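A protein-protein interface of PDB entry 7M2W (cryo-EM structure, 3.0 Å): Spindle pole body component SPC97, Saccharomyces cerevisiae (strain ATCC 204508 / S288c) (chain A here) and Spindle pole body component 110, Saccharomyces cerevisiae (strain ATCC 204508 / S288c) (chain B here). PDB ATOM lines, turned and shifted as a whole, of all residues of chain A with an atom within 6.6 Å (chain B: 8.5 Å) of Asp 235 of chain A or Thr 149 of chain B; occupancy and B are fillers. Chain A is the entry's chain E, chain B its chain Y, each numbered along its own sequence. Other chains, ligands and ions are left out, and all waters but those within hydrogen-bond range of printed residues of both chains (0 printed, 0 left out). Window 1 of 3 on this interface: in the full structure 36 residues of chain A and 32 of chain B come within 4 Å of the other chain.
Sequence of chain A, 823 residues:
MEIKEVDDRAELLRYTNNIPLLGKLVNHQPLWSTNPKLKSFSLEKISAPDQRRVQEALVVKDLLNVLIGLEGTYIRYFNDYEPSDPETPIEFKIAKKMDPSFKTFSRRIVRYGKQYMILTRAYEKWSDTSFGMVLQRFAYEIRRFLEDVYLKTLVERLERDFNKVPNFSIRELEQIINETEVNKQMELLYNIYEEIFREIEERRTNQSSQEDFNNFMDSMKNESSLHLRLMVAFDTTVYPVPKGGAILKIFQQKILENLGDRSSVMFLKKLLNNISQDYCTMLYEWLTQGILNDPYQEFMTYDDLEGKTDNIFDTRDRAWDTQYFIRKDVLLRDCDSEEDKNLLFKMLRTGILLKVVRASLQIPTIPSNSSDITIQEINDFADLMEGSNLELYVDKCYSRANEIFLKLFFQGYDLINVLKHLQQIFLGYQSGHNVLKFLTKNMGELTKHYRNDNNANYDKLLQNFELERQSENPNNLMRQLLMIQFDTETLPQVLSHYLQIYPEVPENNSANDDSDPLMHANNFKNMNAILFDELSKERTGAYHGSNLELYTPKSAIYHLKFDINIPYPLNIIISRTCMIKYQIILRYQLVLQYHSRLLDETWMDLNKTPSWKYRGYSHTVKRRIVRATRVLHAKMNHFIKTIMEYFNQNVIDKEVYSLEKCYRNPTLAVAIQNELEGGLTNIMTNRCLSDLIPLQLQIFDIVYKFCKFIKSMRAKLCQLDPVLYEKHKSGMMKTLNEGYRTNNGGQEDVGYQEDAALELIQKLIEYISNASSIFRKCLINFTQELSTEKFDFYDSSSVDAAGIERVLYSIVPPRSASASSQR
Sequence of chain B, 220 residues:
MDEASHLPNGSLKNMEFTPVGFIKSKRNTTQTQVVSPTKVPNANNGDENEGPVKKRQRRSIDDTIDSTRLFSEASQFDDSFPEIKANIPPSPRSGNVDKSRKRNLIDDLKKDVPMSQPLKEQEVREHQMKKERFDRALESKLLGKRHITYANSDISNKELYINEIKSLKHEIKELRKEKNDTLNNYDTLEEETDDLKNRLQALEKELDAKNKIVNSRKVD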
ATOM      1  N   ALA A 233       5.543 -13.580  14.594  1.00  0.00           N
ATOM      2  CA  ALA A 233       4.876 -12.638  13.711  1.00  0.00           C
ATOM      3  C   ALA A 233       3.827 -13.390  12.910  1.00  0.00           C
ATOM      4  O   ALA A 233       3.984 -14.578  12.622  1.00  0.00           O
ATOM      5  CB  ALA A 233       5.862 -11.941  12.766  1.00  0.00           C
ATOM      6  N   PHE A 234       2.752 -12.695  12.561  1.00  0.00           N
ATOM      7  CA  PHE A 234       1.750 -13.245  11.664  1.00  0.00           C
ATOM      8  C   PHE A 234       2.192 -13.057  10.222  1.00  0.00           C
ATOM      9  O   PHE A 234       2.633 -11.974   9.832  1.00  0.00           O
ATOM     10  CB  PHE A 234       0.389 -12.584  11.883  1.00  0.00           C
ATOM     11  CG  PHE A 234      -0.313 -13.035  13.128  1.00  0.00           C
ATOM     12  CD1 PHE A 234       0.079 -14.188  13.781  1.00  0.00           C
ATOM     13  CD2 PHE A 234      -1.373 -12.305  13.643  1.00  0.00           C
ATOM     14  CE1 PHE A 234      -0.570 -14.606  14.926  1.00  0.00           C
ATOM     15  CE2 PHE A 234      -2.025 -12.716  14.789  1.00  0.00           C
ATOM     16  CZ  PHE A 234      -1.623 -13.869  15.431  1.00  0.00           C
ATOM     17  N   ASP A 235       2.073 -14.121   9.435  1.00  0.00           N
ATOM     18  CA  ASP A 235       2.413 -14.104   8.018  1.00  0.00           C
ATOM     19  C   ASP A 235       1.105 -14.085   7.241  1.00  0.00           C
ATOM     20  O   ASP A 235       0.571 -15.141   6.890  1.00  0.00           O
ATOM     21  CB  ASP A 235       3.269 -15.312   7.646  1.00  0.00           C
ATOM     22  CG  ASP A 235       3.844 -15.216   6.247  1.00  0.00           C
ATOM     23  OD1 ASP A 235       3.307 -14.452   5.419  1.00  0.00           O
ATOM     24  OD2 ASP A 235       4.847 -15.906   5.974  1.00  0.00           O
ATOM     25  N   THR A 236       0.593 -12.885   6.972  1.00  0.00           N
ATOM     26  CA  THR A 236      -0.705 -12.715   6.338  1.00  0.00           C
ATOM     27  C   THR A 236      -0.608 -12.726   4.814  1.00  0.00           C
ATOM     28  O   THR A 236      -1.486 -12.187   4.134  1.00  0.00           O
ATOM     29  CB  THR A 236      -1.357 -11.420   6.830  1.00  0.00           C
ATOM     30  OG1 THR A 236      -1.040 -11.234   8.214  1.00  0.00           O
ATOM     31  CG2 THR A 236      -2.872 -11.493   6.703  1.00  0.00           C
ATOM     32  N   THR A 237       0.445 -13.325   4.265  1.00  0.00           N
ATOM     33  CA  THR A 237       0.556 -13.437   2.819  1.00  0.00           C
ATOM     34  C   THR A 237      -0.520 -14.371   2.286  1.00  0.00           C
ATOM     35  O   THR A 237      -0.550 -15.558   2.623  1.00  0.00           O
ATOM     36  CB  THR A 237       1.938 -13.951   2.423  1.00  0.00           C
ATOM     37  OG1 THR A 237       2.947 -13.209   3.119  1.00  0.00           O
ATOM     38  CG2 THR A 237       2.149 -13.792   0.928  1.00  0.00           C
ATOM     39  N   VAL A 238      -1.404 -13.832   1.454  1.00  0.00           N
ATOM     40  CA  VAL A 238      -2.467 -14.607   0.828  1.00  0.00           C
ATOM     41  C   VAL A 238      -1.884 -15.256  -0.418  1.00  0.00           C
ATOM     42  O   VAL A 238      -1.789 -14.622  -1.475  1.00  0.00           O
ATOM     43  CB  VAL A 238      -3.679 -13.727   0.490  1.00  0.00           C
ATOM     44  CG1 VAL A 238      -4.708 -14.516  -0.297  1.00  0.00           C
ATOM     45  CG2 VAL A 238      -4.292 -13.175   1.763  1.00  0.00           C
ATOM     46  N   TYR A 239      -1.477 -16.512  -0.285  1.00  0.00           N
ATOM     47  CA  TYR A 239      -0.768 -17.225  -1.331  1.00  0.00           C
ATOM     48  C   TYR A 239      -1.645 -17.377  -2.573  1.00  0.00           C
ATOM     49  O   TYR A 239      -2.874 -17.319  -2.484  1.00  0.00           O
ATOM     50  CB  TYR A 239      -0.333 -18.595  -0.824  1.00  0.00           C
ATOM     51  CG  TYR A 239       0.801 -18.528   0.170  1.00  0.00           C
ATOM     52  CD1 TYR A 239       0.684 -19.104   1.426  1.00  0.00           C
ATOM     53  CD2 TYR A 239       1.984 -17.877  -0.143  1.00  0.00           C
ATOM     54  CE1 TYR A 239       1.719 -19.040   2.337  1.00  0.00           C
ATOM     55  CE2 TYR A 239       3.021 -17.807   0.760  1.00  0.00           C
ATOM     56  CZ  TYR A 239       2.885 -18.389   1.999  1.00  0.00           C
ATOM     57  OH  TYR A 239       3.921 -18.320   2.902  1.00  0.00           O
ATOM     58  N   TYR A 302       6.251 -21.604  10.606  1.00  0.00           N
ATOM     59  CA  TYR A 302       7.584 -21.878  10.090  1.00  0.00           C
ATOM     60  C   TYR A 302       8.576 -20.938  10.753  1.00  0.00           C
ATOM     61  O   TYR A 302       8.200 -20.030  11.497  1.00  0.00           O
ATOM     62  CB  TYR A 302       7.648 -21.728   8.567  1.00  0.00           C
ATOM     63  CG  TYR A 302       7.452 -20.315   8.071  1.00  0.00           C
ATOM     64  CD1 TYR A 302       8.523 -19.570   7.605  1.00  0.00           C
ATOM     65  CD2 TYR A 302       6.195 -19.732   8.050  1.00  0.00           C
ATOM     66  CE1 TYR A 302       8.351 -18.283   7.144  1.00  0.00           C
ATOM     67  CE2 TYR A 302       6.013 -18.448   7.587  1.00  0.00           C
ATOM     68  CZ  TYR A 302       7.094 -17.726   7.138  1.00  0.00           C
ATOM     69  OH  TYR A 302       6.917 -16.444   6.677  1.00  0.00           O
ATOM     70  N   PHE A 325       7.095 -17.782  12.527  1.00  0.00           N
ATOM     71  CA  PHE A 325       5.994 -17.064  11.912  1.00  0.00           C
ATOM     72  C   PHE A 325       4.773 -17.970  11.905  1.00  0.00           C
ATOM     73  O   PHE A 325       4.887 -19.185  12.076  1.00  0.00           O
ATOM     74  CB  PHE A 325       6.326 -16.627  10.481  1.00  0.00           C
ATOM     75  CG  PHE A 325       7.558 -15.771  10.364  1.00  0.00           C
ATOM     76  CD1 PHE A 325       8.819 -16.303  10.575  1.00  0.00           C
ATOM     77  CD2 PHE A 325       7.454 -14.434  10.037  1.00  0.00           C
ATOM     78  CE1 PHE A 325       9.945 -15.517  10.464  1.00  0.00           C
ATOM     79  CE2 PHE A 325       8.577 -13.644   9.923  1.00  0.00           C
ATOM     80  CZ  PHE A 325       9.824 -14.187  10.138  1.00  0.00           C
ATOM     81  N   ILE A 326       3.601 -17.376  11.713  1.00  0.00           N
ATOM     82  CA  ILE A 326       2.356 -18.123  11.592  1.00  0.00           C
ATOM     83  C   ILE A 326       1.709 -17.754  10.268  1.00  0.00           C
ATOM     84  O   ILE A 326       1.379 -16.587  10.032  1.00  0.00           O
ATOM     85  CB  ILE A 326       1.407 -17.852  12.768  1.00  0.00           C
ATOM     86  CG1 ILE A 326       1.986 -18.427  14.060  1.00  0.00           C
ATOM     87  CG2 ILE A 326       0.038 -18.441  12.493  1.00  0.00           C
ATOM     88  CD1 ILE A 326       1.221 -18.027  15.296  1.00  0.00           C
ATOM     89  N   ARG A 327       1.529 -18.749   9.403  1.00  0.00           N
ATOM     90  CA  ARG A 327       0.870 -18.551   8.116  1.00  0.00           C
ATOM     91  C   ARG A 327      -0.627 -18.479   8.372  1.00  0.00           C
ATOM     92  O   ARG A 327      -1.295 -19.492   8.580  1.00  0.00           O
ATOM     93  CB  ARG A 327       1.222 -19.673   7.152  1.00  0.00           C
ATOM     94  CG  ARG A 327       2.642 -19.629   6.627  1.00  0.00           C
ATOM     95  CD  ARG A 327       2.816 -20.544   5.428  1.00  0.00           C
ATOM     96  NE  ARG A 327       4.213 -20.637   5.014  1.00  0.00           N
ATOM     97  CZ  ARG A 327       5.063 -21.548   5.471  1.00  0.00           C
ATOM     98  NH1 ARG A 327       4.657 -22.445   6.355  1.00  0.00           N
ATOM     99  NH2 ARG A 327       6.317 -21.564   5.044  1.00  0.00           N
ATOM    100  N   LYS A 328      -1.165 -17.259   8.359  1.00  0.00           N
ATOM    101  CA  LYS A 328      -2.592 -17.083   8.606  1.00  0.00           C
ATOM    102  C   LYS A 328      -3.421 -17.664   7.470  1.00  0.00           C
ATOM    103  O   LYS A 328      -4.633 -17.863   7.610  1.00  0.00           O
ATOM    104  CB  LYS A 328      -2.911 -15.601   8.802  1.00  0.00           C
ATOM    105  CG  LYS A 328      -4.209 -15.342   9.545  1.00  0.00           C
ATOM    106  CD  LYS A 328      -4.390 -13.867   9.848  1.00  0.00           C
ATOM    107  CE  LYS A 328      -5.690 -13.612  10.594  1.00  0.00           C
ATOM    108  NZ  LYS A 328      -5.854 -14.511  11.769  1.00  0.00           N
ATOM    109  N   ASP A 329      -2.784 -17.946   6.334  1.00  0.00           N
ATOM    110  CA  ASP A 329      -3.492 -18.501   5.189  1.00  0.00           C
ATOM    111  C   ASP A 329      -3.789 -19.985   5.332  1.00  0.00           C
ATOM    112  O   ASP A 329      -4.878 -20.418   4.940  1.00  0.00           O
ATOM    113  CB  ASP A 329      -2.691 -18.266   3.912  1.00  0.00           C
ATOM    114  CG  ASP A 329      -3.528 -18.442   2.667  1.00  0.00           C
ATOM    115  OD1 ASP A 329      -4.755 -18.216   2.742  1.00  0.00           O
ATOM    116  OD2 ASP A 329      -2.966 -18.810   1.616  1.00  0.00           O
ATOM    117  N   ARG B 146       5.721  -7.798  17.884  1.00  0.00           N
ATOM    118  CA  ARG B 146       4.382  -8.288  17.500  1.00  0.00           C
ATOM    119  C   ARG B 146       3.958  -7.696  16.141  1.00  0.00           C
ATOM    120  O   ARG B 146       3.138  -6.786  16.060  1.00  0.00           O
ATOM    121  CB  ARG B 146       3.429  -7.987  18.678  1.00  0.00           C
ATOM    122  CG  ARG B 146       2.098  -8.758  18.675  1.00  0.00           C
ATOM    123  CD  ARG B 146       1.018  -8.288  17.692  1.00  0.00           C
ATOM    124  NE  ARG B 146       0.803  -6.832  17.773  1.00  0.00           N
ATOM    125  CZ  ARG B 146      -0.008  -6.162  18.563  1.00  0.00           C
ATOM    126  NH1 ARG B 146      -0.877  -6.738  19.338  1.00  0.00           N
ATOM    127  NH2 ARG B 146       0.038  -4.870  18.583  1.00  0.00           N
ATOM    128  N   HIS B 147       4.569  -8.191  15.070  1.00  0.00           N
ATOM    129  CA  HIS B 147       4.426  -7.703  13.690  1.00  0.00           C
ATOM    130  C   HIS B 147       3.511  -8.576  12.815  1.00  0.00           C
ATOM    131  O   HIS B 147       3.199  -9.722  13.132  1.00  0.00           O
ATOM    132  CB  HIS B 147       5.824  -7.581  13.053  1.00  0.00           C
ATOM    133  CG  HIS B 147       6.667  -6.463  13.615  1.00  0.00           C
ATOM    134  ND1 HIS B 147       6.362  -5.106  13.515  1.00  0.00           N
ATOM    135  CD2 HIS B 147       7.883  -6.598  14.218  1.00  0.00           C
ATOM    136  CE1 HIS B 147       7.387  -4.454  14.089  1.00  0.00           C
ATOM    137  NE2 HIS B 147       8.315  -5.324  14.517  1.00  0.00           N
ATOM    138  N   ILE B 148       3.166  -8.037  11.648  1.00  0.00           N
ATOM    139  CA  ILE B 148       2.637  -8.767  10.486  1.00  0.00           C
ATOM    140  C   ILE B 148       3.641  -8.664   9.325  1.00  0.00           C
ATOM    141  O   ILE B 148       4.377  -7.683   9.222  1.00  0.00           O
ATOM    142  CB  ILE B 148       1.216  -8.290  10.108  1.00  0.00           C
ATOM    143  CG1 ILE B 148       1.182  -6.854   9.541  1.00  0.00           C
ATOM    144  CG2 ILE B 148       0.270  -8.445  11.309  1.00  0.00           C
ATOM    145  CD1 ILE B 148      -0.199  -6.413   9.045  1.00  0.00           C
ATOM    146  N   THR B 149       3.719  -9.683   8.470  1.00  0.00           N
ATOM    147  CA  THR B 149       4.741  -9.792   7.410  1.00  0.00           C
ATOM    148  C   THR B 149       4.201 -10.446   6.129  1.00  0.00           C
ATOM    149  O   THR B 149       3.122 -11.042   6.138  1.00  0.00           O
ATOM    150  CB  THR B 149       5.997 -10.498   7.957  1.00  0.00           C
ATOM    151  OG1 THR B 149       7.072 -10.349   7.064  1.00  0.00           O
ATOM    152  CG2 THR B 149       5.818 -11.996   8.187  1.00  0.00           C
ATOM    153  N   TYR B 150       4.931 -10.308   5.020  1.00  0.00           N
ATOM    154  CA  TYR B 150       4.579 -10.810   3.687  1.00  0.00           C
ATOM    155  C   TYR B 150       5.791 -11.478   3.006  1.00  0.00           C
ATOM    156  O   TYR B 150       6.913 -10.980   3.106  1.00  0.00           O
ATOM    157  CB  TYR B 150       4.019  -9.637   2.873  1.00  0.00           C
ATOM    158  CG  TYR B 150       3.552  -9.977   1.472  1.00  0.00           C
ATOM    159  CD1 TYR B 150       2.211 -10.324   1.241  1.00  0.00           C
ATOM    160  CD2 TYR B 150       4.452  -9.914   0.396  1.00  0.00           C
ATOM    161  CE1 TYR B 150       1.772 -10.615  -0.064  1.00  0.00           C
ATOM    162  CE2 TYR B 150       4.019 -10.214  -0.907  1.00  0.00           C
ATOM    163  CZ  TYR B 150       2.678 -10.569  -1.140  1.00  0.00           C
ATOM    164  OH  TYR B 150       2.256 -10.865  -2.395  1.00  0.00           O
ATOM    165  N   ALA B 151       5.586 -12.610   2.332  1.00  0.00           N
ATOM    166  CA  ALA B 151       6.640 -13.442   1.744  1.00  0.00           C
ATOM    167  C   ALA B 151       7.249 -12.863   0.448  1.00  0.00           C
ATOM    168  O   ALA B 151       6.555 -12.239  -0.350  1.00  0.00           O
ATOM    169  CB  ALA B 151       6.068 -14.844   1.511  1.00  0.00           C
ATOM    170  N   ASN B 152       8.541 -13.117   0.210  1.00  0.00           N
ATOM    171  CA  ASN B 152       9.322 -12.511  -0.886  1.00  0.00           C
ATOM    172  C   ASN B 152       9.997 -13.516  -1.850  1.00  0.00           C
ATOM    173  O   ASN B 152      10.750 -13.102  -2.731  1.00  0.00           O
ATOM    174  CB  ASN B 152      10.348 -11.533  -0.277  1.00  0.00           C
ATOM    175  CG  ASN B 152       9.714 -10.405   0.517  1.00  0.00           C
ATOM    176  OD1 ASN B 152       8.943  -9.613   0.007  1.00  0.00           O
ATOM    177  ND2 ASN B 152      10.028 -10.284   1.781  1.00  0.00           N
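Of chain B, only Thr 149 comes within 4 Å of Asp 235 of chain A.
Of the printed residues of chain A, Thr 149 of chain B touches Phe 234, Asp 235, Thr 236, Thr 237 and Phe 325.
Of the printed residues of chain B, Phe 234 of chain A touches His 147 (3.1 Å), Ile 148 (3.3 Å) and Thr 149 (2.9 Å).
Of the printed residues of chain A, His 147 of chain B touches Ala 233 (3.4 Å) and Phe 234 (3.1 Å).
Of the printed residues of chain B, Ala 233 of chain A touches His 147.
Asp 329 of chain A touches none of the printed residues of chain B.
Tyr 302 of chain A touches none of the printed residues of chain B.
The nearest printed residue of chain B that does not touch Phe 325 of chain A is Ile 148 of chain B (7.0 Å).
Hydrophobic or aromatic side chains of chain A that line the printed part of chain B: Ala 233 and Phe 325.
Along chain A the printed residues that touch a printed residue of chain B span positions 233 to 325.
Ala 233 of chain A touches His 147 of chain B (CA to O, 3.4 Å).
Ile 148 of chain B touches Phe 234 of chain A (CA to O, 3.3 Å).
Thr 149 of chain B touches Thr 237 of chain A.
Thr 237 of chain A touches Tyr 150 of chain B.
Phe 325 of chain A touches Thr 149 of chain B.
The backbone carbonyl oxygen (O) of Ala 233 of chain A lies within hydrogen-bond range of the backbone NH (N) of Ile 326 of chain A (3.0 Å).
The side-chain carboxylate (OD1) of Asp 235 of chain A sits at hydrogen-bond distance from the side-chain hydroxyl (OG1) of Thr 237 of chain A, at 2.6 Å.
The backbone NH (N) of Asp 235 of chain A is in hydrogen-bond range of the backbone carbonyl oxygen (O) of Ile 326 of chain A, 2.6 Å away.
The backbone carbonyl oxygen of Asp 235 of chain A lies within hydrogen-bond range of the backbone NH of Lys 328 of chain A (3.1 Å).
The backbone carbonyl oxygen of Tyr 302 of chain A lies within hydrogen-bond range of the backbone NH of Phe 325 of chain A, 2.7 Å away.
The side-chain amide nitrogen (ND2) of Asn 152 of chain B sits at hydrogen-bond distance from the backbone carbonyl oxygen (O) of Tyr 150 of chain B (3.5 Å).
The backbone NH (N) of Phe 234 of chain A lies within hydrogen-bond range of the backbone carbonyl oxygen (O) of His 147 of chain B, at 3.1 Å.
The backbone carbonyl oxygen (O) of Phe 234 of chain A lies within hydrogen-bond range of the backbone NH (N) of Thr 149 of chain B (2.9 Å).
N of Thr 236 of chain A lies within hydrogen-bond range of O of Thr 149 of chain B (3.2 Å).
OG1 of Thr 237 of chain A is in hydrogen-bond range of N of Ala 151 of chain B, 2.8 Å away.
The backbone carbonyl oxygen (O) of Thr 149 of chain B sits close to the side-chain carboxylate (OD1) of Asp 235 of chain A (3.5 Å).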
